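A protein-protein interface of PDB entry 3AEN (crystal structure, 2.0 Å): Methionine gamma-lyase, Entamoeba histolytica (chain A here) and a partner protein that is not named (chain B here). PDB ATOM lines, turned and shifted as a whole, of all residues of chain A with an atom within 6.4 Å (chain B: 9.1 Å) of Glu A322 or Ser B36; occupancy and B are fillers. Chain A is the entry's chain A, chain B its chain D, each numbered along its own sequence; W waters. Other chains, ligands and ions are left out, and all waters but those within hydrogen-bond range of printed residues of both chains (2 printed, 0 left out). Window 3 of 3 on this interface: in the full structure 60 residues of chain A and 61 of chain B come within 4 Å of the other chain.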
ATOM      1  N   ALA A 317      13.130 -35.117  -2.627  1.00  0.00           N
ATOM      2  CA  ALA A 317      11.690 -34.943  -2.629  1.00  0.00           C
ATOM      3  C   ALA A 317      11.371 -33.700  -3.455  1.00  0.00           C
ATOM      4  O   ALA A 317      10.506 -33.750  -4.308  1.00  0.00           O
ATOM      5  CB  ALA A 317      11.150 -34.811  -1.168  1.00  0.00           C
ATOM      6  N   LYS A 318      12.113 -32.609  -3.230  1.00  0.00           N
ATOM      7  CA  LYS A 318      11.937 -31.351  -3.992  1.00  0.00           C
ATOM      8  C   LYS A 318      12.237 -31.562  -5.484  1.00  0.00           C
ATOM      9  O   LYS A 318      11.508 -31.073  -6.341  1.00  0.00           O
ATOM     10  CB  LYS A 318      12.840 -30.254  -3.394  1.00  0.00           C
ATOM     11  CG  LYS A 318      13.097 -29.058  -4.284  1.00  0.00           C
ATOM     12  CD  LYS A 318      14.100 -28.093  -3.620  1.00  0.00           C
ATOM     13  CE  LYS A 318      14.418 -26.819  -4.440  1.00  0.00           C
ATOM     14  NZ  LYS A 318      14.653 -27.031  -5.906  1.00  0.00           N
ATOM     15  N   LYS A 319      13.309 -32.291  -5.795  1.00  0.00           N
ATOM     16  CA  LYS A 319      13.676 -32.556  -7.205  1.00  0.00           C
ATOM     17  C   LYS A 319      12.539 -33.304  -7.927  1.00  0.00           C
ATOM     18  O   LYS A 319      12.120 -32.926  -9.047  1.00  0.00           O
ATOM     19  CB  LYS A 319      15.001 -33.321  -7.295  1.00  0.00           C
ATOM     20  CG  LYS A 319      15.603 -33.356  -8.699  1.00  0.00           C
ATOM     21  CD  LYS A 319      17.080 -33.700  -8.637  1.00  0.00           C
ATOM     22  CE  LYS A 319      17.654 -33.931 -10.028  1.00  0.00           C
ATOM     23  NZ  LYS A 319      19.109 -34.229  -9.892  1.00  0.00           N
ATOM     24  N   LEU A 320      12.026 -34.340  -7.275  1.00  0.00           N
ATOM     25  CA  LEU A 320      10.894 -35.086  -7.806  1.00  0.00           C
ATOM     26  C   LEU A 320       9.660 -34.183  -8.010  1.00  0.00           C
ATOM     27  O   LEU A 320       9.120 -34.107  -9.124  1.00  0.00           O
ATOM     28  CB  LEU A 320      10.528 -36.282  -6.917  1.00  0.00           C
ATOM     29  CG  LEU A 320       9.165 -36.895  -7.290  1.00  0.00           C
ATOM     30  CD1 LEU A 320       9.207 -37.580  -8.667  1.00  0.00           C
ATOM     31  CD2 LEU A 320       8.709 -37.847  -6.239  1.00  0.00           C
ATOM     32  N   MET A 321       9.222 -33.516  -6.945  1.00  0.00           N
ATOM     33  CA  MET A 321       7.996 -32.688  -6.969  1.00  0.00           C
ATOM     34  C   MET A 321       7.996 -31.585  -8.031  1.00  0.00           C
ATOM     35  O   MET A 321       6.930 -31.246  -8.585  1.00  0.00           O
ATOM     36  CB  MET A 321       7.756 -32.059  -5.595  1.00  0.00           C
ATOM     37  CG  MET A 321       7.130 -33.068  -4.626  1.00  0.00           C
ATOM     38  SD  MET A 321       6.841 -32.348  -3.006  1.00  0.00           S
ATOM     39  CE  MET A 321       8.480 -31.835  -2.502  1.00  0.00           C
ATOM     40  N   GLU A 322       9.179 -31.038  -8.305  1.00  0.00           N
ATOM     41  CA  GLU A 322       9.325 -29.889  -9.203  1.00  0.00           C
ATOM     42  C   GLU A 322       9.615 -30.239 -10.663  1.00  0.00           C
ATOM     43  O   GLU A 322       9.791 -29.356 -11.477  1.00  0.00           O
ATOM     44  CB  GLU A 322      10.388 -28.914  -8.633  1.00  0.00           C
ATOM     45  CG  GLU A 322       9.919 -28.355  -7.294  1.00  0.00           C
ATOM     46  CD  GLU A 322      10.931 -27.454  -6.632  1.00  0.00           C
ATOM     47  OE1 GLU A 322      10.675 -27.014  -5.487  1.00  0.00           O
ATOM     48  OE2 GLU A 322      11.980 -27.199  -7.248  1.00  0.00           O
ATOM     49  N   HIS A 323       9.628 -31.524 -11.011  1.00  0.00           N
ATOM     50  CA  HIS A 323       9.998 -31.918 -12.379  1.00  0.00           C
ATOM     51  C   HIS A 323       8.968 -32.888 -12.979  1.00  0.00           C
ATOM     52  O   HIS A 323       9.290 -33.710 -13.843  1.00  0.00           O
ATOM     53  CB  HIS A 323      11.420 -32.476 -12.407  1.00  0.00           C
ATOM     54  CG  HIS A 323      12.467 -31.431 -12.140  1.00  0.00           C
ATOM     55  ND1 HIS A 323      12.891 -31.098 -10.867  1.00  0.00           N
ATOM     56  CD2 HIS A 323      13.138 -30.612 -12.984  1.00  0.00           C
ATOM     57  CE1 HIS A 323      13.785 -30.131 -10.941  1.00  0.00           C
ATOM     58  NE2 HIS A 323      13.945 -29.808 -12.212  1.00  0.00           N
ATOM     59  N   LEU A 324       7.724 -32.744 -12.543  1.00  0.00           N
ATOM     60  CA  LEU A 324       6.603 -33.535 -13.066  1.00  0.00           C
ATOM     61  C   LEU A 324       5.823 -32.746 -14.121  1.00  0.00           C
ATOM     62  O   LEU A 324       5.727 -31.531 -14.045  1.00  0.00           O
ATOM     63  CB  LEU A 324       5.705 -33.953 -11.895  1.00  0.00           C
ATOM     64  CG  LEU A 324       6.421 -34.874 -10.920  1.00  0.00           C
ATOM     65  CD1 LEU A 324       5.680 -35.032  -9.547  1.00  0.00           C
ATOM     66  CD2 LEU A 324       6.712 -36.233 -11.600  1.00  0.00           C
ATOM     67  N   LYS A 325       5.283 -33.414 -15.128  1.00  0.00           N
ATOM     68  CA  LYS A 325       4.541 -32.698 -16.168  1.00  0.00           C
ATOM     69  C   LYS A 325       3.066 -33.018 -16.161  1.00  0.00           C
ATOM     70  O   LYS A 325       2.258 -32.261 -16.670  1.00  0.00           O
ATOM     71  CB  LYS A 325       5.168 -32.924 -17.561  1.00  0.00           C
ATOM     72  CG  LYS A 325       6.423 -32.065 -17.788  1.00  0.00           C
ATOM     73  CD  LYS A 325       7.698 -32.883 -17.507  1.00  0.00           C
ATOM     74  CE  LYS A 325       9.001 -32.075 -17.670  1.00  0.00           C
ATOM     75  NZ  LYS A 325       9.538 -31.405 -16.414  1.00  0.00           N
ATOM     76  N   LEU A 329       1.633 -29.716  -8.604  1.00  0.00           N
ATOM     77  CA  LEU A 329       2.053 -29.336  -7.283  1.00  0.00           C
ATOM     78  C   LEU A 329       1.005 -28.404  -6.664  1.00  0.00           C
ATOM     79  O   LEU A 329       0.880 -27.232  -7.045  1.00  0.00           O
ATOM     80  CB  LEU A 329       3.469 -28.692  -7.351  1.00  0.00           C
ATOM     81  CG  LEU A 329       4.192 -28.374  -6.020  1.00  0.00           C
ATOM     82  CD1 LEU A 329       4.465 -29.621  -5.167  1.00  0.00           C
ATOM     83  CD2 LEU A 329       5.510 -27.556  -6.269  1.00  0.00           C
ATOM     84  N   MET A 346       3.755 -27.894   3.927  1.00  0.00           N
ATOM     85  CA  MET A 346       2.441 -27.483   3.385  1.00  0.00           C
ATOM     86  C   MET A 346       1.198 -27.870   4.254  1.00  0.00           C
ATOM     87  O   MET A 346       0.865 -27.124   5.164  1.00  0.00           O
ATOM     88  CB  MET A 346       2.287 -27.910   1.905  1.00  0.00           C
ATOM     89  CG  MET A 346       3.449 -27.468   0.958  1.00  0.00           C
ATOM     90  SD  MET A 346       3.291 -28.106  -0.767  1.00  0.00           S
ATOM     91  CE  MET A 346       4.763 -27.476  -1.506  1.00  0.00           C
ATOM     92  N   CYS B  33      -2.307 -23.926  -7.717  1.00  0.00           N
ATOM     93  CA  CYS B  33      -1.027 -24.552  -8.058  1.00  0.00           C
ATOM     94  C   CYS B  33       0.114 -23.742  -7.481  1.00  0.00           C
ATOM     95  O   CYS B  33      -0.017 -22.521  -7.308  1.00  0.00           O
ATOM     96  CB  CYS B  33      -0.877 -24.592  -9.599  1.00  0.00           C
ATOM     97  SG  CYS B  33      -2.358 -25.390 -10.315  1.00  0.00           S
ATOM     98  N   PHE B  34       1.219 -24.425  -7.172  1.00  0.00           N
ATOM     99  CA  PHE B  34       2.428 -23.785  -6.711  1.00  0.00           C
ATOM    100  C   PHE B  34       3.476 -23.801  -7.840  1.00  0.00           C
ATOM    101  O   PHE B  34       3.533 -24.759  -8.599  1.00  0.00           O
ATOM    102  CB  PHE B  34       2.981 -24.509  -5.470  1.00  0.00           C
ATOM    103  CG  PHE B  34       2.085 -24.402  -4.245  1.00  0.00           C
ATOM    104  CD1 PHE B  34       1.364 -23.228  -3.982  1.00  0.00           C
ATOM    105  CD2 PHE B  34       1.970 -25.462  -3.356  1.00  0.00           C
ATOM    106  CE1 PHE B  34       0.529 -23.113  -2.854  1.00  0.00           C
ATOM    107  CE2 PHE B  34       1.153 -25.352  -2.200  1.00  0.00           C
ATOM    108  CZ  PHE B  34       0.449 -24.175  -1.942  1.00  0.00           C
ATOM    109  N   ASP B  35       4.292 -22.743  -7.927  1.00  0.00           N
ATOM    110  CA  ASP B  35       5.426 -22.681  -8.873  1.00  0.00           C
ATOM    111  C   ASP B  35       6.570 -23.610  -8.454  1.00  0.00           C
ATOM    112  O   ASP B  35       7.354 -24.017  -9.292  1.00  0.00           O
ATOM    113  CB  ASP B  35       6.014 -21.264  -8.965  1.00  0.00           C
ATOM    114  CG  ASP B  35       4.976 -20.206  -9.364  1.00  0.00           C
ATOM    115  OD1 ASP B  35       4.172 -20.455 -10.263  1.00  0.00           O
ATOM    116  OD2 ASP B  35       4.975 -19.123  -8.757  1.00  0.00           O
ATOM    117  N   SER B  36       6.679 -23.910  -7.156  1.00  0.00           N
ATOM    118  CA  SER B  36       7.809 -24.677  -6.631  1.00  0.00           C
ATOM    119  C   SER B  36       7.458 -25.001  -5.186  1.00  0.00           C
ATOM    120  O   SER B  36       6.514 -24.418  -4.623  1.00  0.00           O
ATOM    121  CB  SER B  36       9.097 -23.823  -6.637  1.00  0.00           C
ATOM    122  OG  SER B  36       8.972 -22.778  -5.675  1.00  0.00           O
ATOM    123  N   THR B  37       8.209 -25.916  -4.590  1.00  0.00           N
ATOM    124  CA  THR B  37       8.027 -26.241  -3.174  1.00  0.00           C
ATOM    125  C   THR B  37       8.182 -24.998  -2.272  1.00  0.00           C
ATOM    126  O   THR B  37       7.343 -24.736  -1.386  1.00  0.00           O
ATOM    127  CB  THR B  37       9.032 -27.324  -2.730  1.00  0.00           C
ATOM    128  OG1 THR B  37       8.888 -28.443  -3.607  1.00  0.00           O
ATOM    129  CG2 THR B  37       8.723 -27.785  -1.276  1.00  0.00           C
ATOM    130  N   GLN B  38       9.243 -24.237  -2.524  1.00  0.00           N
ATOM    131  CA  GLN B  38       9.539 -23.029  -1.778  1.00  0.00           C
ATOM    132  C   GLN B  38       8.405 -22.022  -1.820  1.00  0.00           C
ATOM    133  O   GLN B  38       8.045 -21.452  -0.794  1.00  0.00           O
ATOM    134  CB  GLN B  38      10.850 -22.369  -2.278  1.00  0.00           C
ATOM    135  CG  GLN B  38      11.349 -21.246  -1.377  1.00  0.00           C
ATOM    136  CD  GLN B  38      11.488 -21.696   0.078  1.00  0.00           C
ATOM    137  OE1 GLN B  38      12.242 -22.625   0.397  1.00  0.00           O
ATOM    138  NE2 GLN B  38      10.736 -21.054   0.962  1.00  0.00           N
ATOM    139  N   GLN B  39       7.862 -21.775  -2.999  1.00  0.00           N
ATOM    140  CA  GLN B  39       6.768 -20.813  -3.114  1.00  0.00           C
ATOM    141  C   GLN B  39       5.493 -21.274  -2.343  1.00  0.00           C
ATOM    142  O   GLN B  39       4.828 -20.459  -1.689  1.00  0.00           O
ATOM    143  CB  GLN B  39       6.492 -20.504  -4.599  1.00  0.00           C
ATOM    144  CG  GLN B  39       5.421 -19.407  -4.846  1.00  0.00           C
ATOM    145  CD  GLN B  39       4.061 -19.986  -5.207  1.00  0.00           C
ATOM    146  OE1 GLN B  39       3.958 -21.137  -5.635  1.00  0.00           O
ATOM    147  NE2 GLN B  39       3.013 -19.182  -5.067  1.00  0.00           N
ATOM    148  N   GLY B  40       5.180 -22.572  -2.404  1.00  0.00           N
ATOM    149  CA  GLY B  40       4.106 -23.147  -1.580  1.00  0.00           C
ATOM    150  C   GLY B  40       4.405 -23.003  -0.082  1.00  0.00           C
ATOM    151  O   GLY B  40       3.592 -22.477   0.668  1.00  0.00           O
ATOM    152  N   ALA B  41       5.593 -23.436   0.335  1.00  0.00           N
ATOM    153  CA  ALA B  41       6.039 -23.256   1.730  1.00  0.00           C
ATOM    154  C   ALA B  41       5.919 -21.801   2.215  1.00  0.00           C
ATOM    155  O   ALA B  41       5.417 -21.546   3.315  1.00  0.00           O
ATOM    156  CB  ALA B  41       7.469 -23.749   1.896  1.00  0.00           C
ATOM    157  N   ASP B  42       6.390 -20.852   1.402  1.00  0.00           N
ATOM    158  CA  ASP B  42       6.305 -19.432   1.733  1.00  0.00           C
ATOM    159  C   ASP B  42       4.844 -18.982   1.966  1.00  0.00           C
ATOM    160  O   ASP B  42       4.533 -18.298   2.968  1.00  0.00           O
ATOM    161  CB  ASP B  42       6.956 -18.592   0.630  1.00  0.00           C
ATOM    162  CG  ASP B  42       8.477 -18.637   0.682  1.00  0.00           C
ATOM    163  OD1 ASP B  42       9.043 -19.294   1.590  1.00  0.00           O
ATOM    164  OD2 ASP B  42       9.106 -18.019  -0.201  1.00  0.00           O
ATOM    165  N   LEU B  43       3.955 -19.375   1.056  1.00  0.00           N
ATOM    166  CA  LEU B  43       2.550 -19.002   1.185  1.00  0.00           C
ATOM    167  C   LEU B  43       1.935 -19.527   2.490  1.00  0.00           C
ATOM    168  O   LEU B  43       1.211 -18.797   3.170  1.00  0.00           O
ATOM    169  CB  LEU B  43       1.732 -19.450  -0.034  1.00  0.00           C
ATOM    170  CG  LEU B  43       1.939 -18.679  -1.345  1.00  0.00           C
ATOM    171  CD1 LEU B  43       0.933 -19.192  -2.369  1.00  0.00           C
ATOM    172  CD2 LEU B  43       1.801 -17.157  -1.157  1.00  0.00           C
ATOM    173  N   PHE B  44       2.205 -20.783   2.835  1.00  0.00           N
ATOM    174  CA  PHE B  44       1.727 -21.318   4.113  1.00  0.00           C
ATOM    175  C   PHE B  44       2.279 -20.559   5.355  1.00  0.00           C
ATOM    176  O   PHE B  44       1.685 -20.614   6.429  1.00  0.00           O
ATOM    177  CB  PHE B  44       2.040 -22.809   4.206  1.00  0.00           C
ATOM    178  CG  PHE B  44       0.923 -23.701   3.678  1.00  0.00           C
ATOM    179  CD1 PHE B  44       0.994 -24.242   2.382  1.00  0.00           C
ATOM    180  CD2 PHE B  44      -0.200 -23.961   4.469  1.00  0.00           C
ATOM    181  CE1 PHE B  44      -0.028 -25.073   1.888  1.00  0.00           C
ATOM    182  CE2 PHE B  44      -1.237 -24.815   3.984  1.00  0.00           C
ATOM    183  CZ  PHE B  44      -1.153 -25.336   2.688  1.00  0.00           C
HETATM  184  O   HOH W   1      11.519 -24.907  -4.245  1.00  0.00           O
HETATM  185  O   HOH W   2       1.832 -26.519  -9.828  1.00  0.00           O
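Hydrophobic or aromatic side chains of chain B within 4 Å of the printed part of chain A: Phe B34 and Phe B44. Among the printed residues, 10 pairs touch across the chains.
The side-chain carboxylate of Glu A322 sits at hydrogen-bond distance from the backbone NH of Thr B37 (2.8 Å). O of Leu A329 sits at hydrogen-bond distance from N of Phe B34 (2.8 Å).
His A323 touches none of the printed residues of chain B. Of the printed residues of chain B, Met A346 touches Phe B34, Thr B37 and Phe B44. Of the printed residues of chain A, Cys B33 touches Leu A329 (3.4 Å). Printed residues of chain A within 4 Å of Phe B34: Leu A329 and Met A346. Ser B36 touches just these residues of chain A: Glu A322 and Leu A329. Ala B41 touches none of the printed residues of chain A. The nearest residue of chain A that does not touch Ser B36 is Met A346 (4.7 Å).
Among the printed residues, merely in contact across the chains: Met A346 with Phe B44 (3.3 Å), Leu A329 with Ser B36 (3.4 Å), Leu A329 with Cys B33 (3.4 Å), Leu A329 with Thr B37 (3.6 Å), Met A321 with Thr B37 (3.6 Å), Glu A322 with Ser B36 (3.7 Å), Met A346 with Thr B37 (3.8 Å) and Met A346 with Phe B34 (3.8 Å).
Water W1 lies within hydrogen-bond range of the side-chain carboxylate of Glu A322 (2.6 Å), the backbone NH of Gln B38 (2.9 Å) and the backbone NH of Thr B37 (3.5 Å). Water W2 lies within hydrogen-bond range of O of Phe B34 (2.7 Å) and O of Leu A329 (3.0 Å).
The side-chain carboxylate (OE2) of Glu A322 lies within salt-bridge range of the side-chain amino group (NZ) of Lys A318, at 3.0 Å. OG of Ser B36 sits close to N of Gln B38, 3.5 Å away. The side-chain hydroxyl (OG) of Ser B36 is in hydrogen-bond range of the backbone NH (N) of Gln B39, 3.1 Å away.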
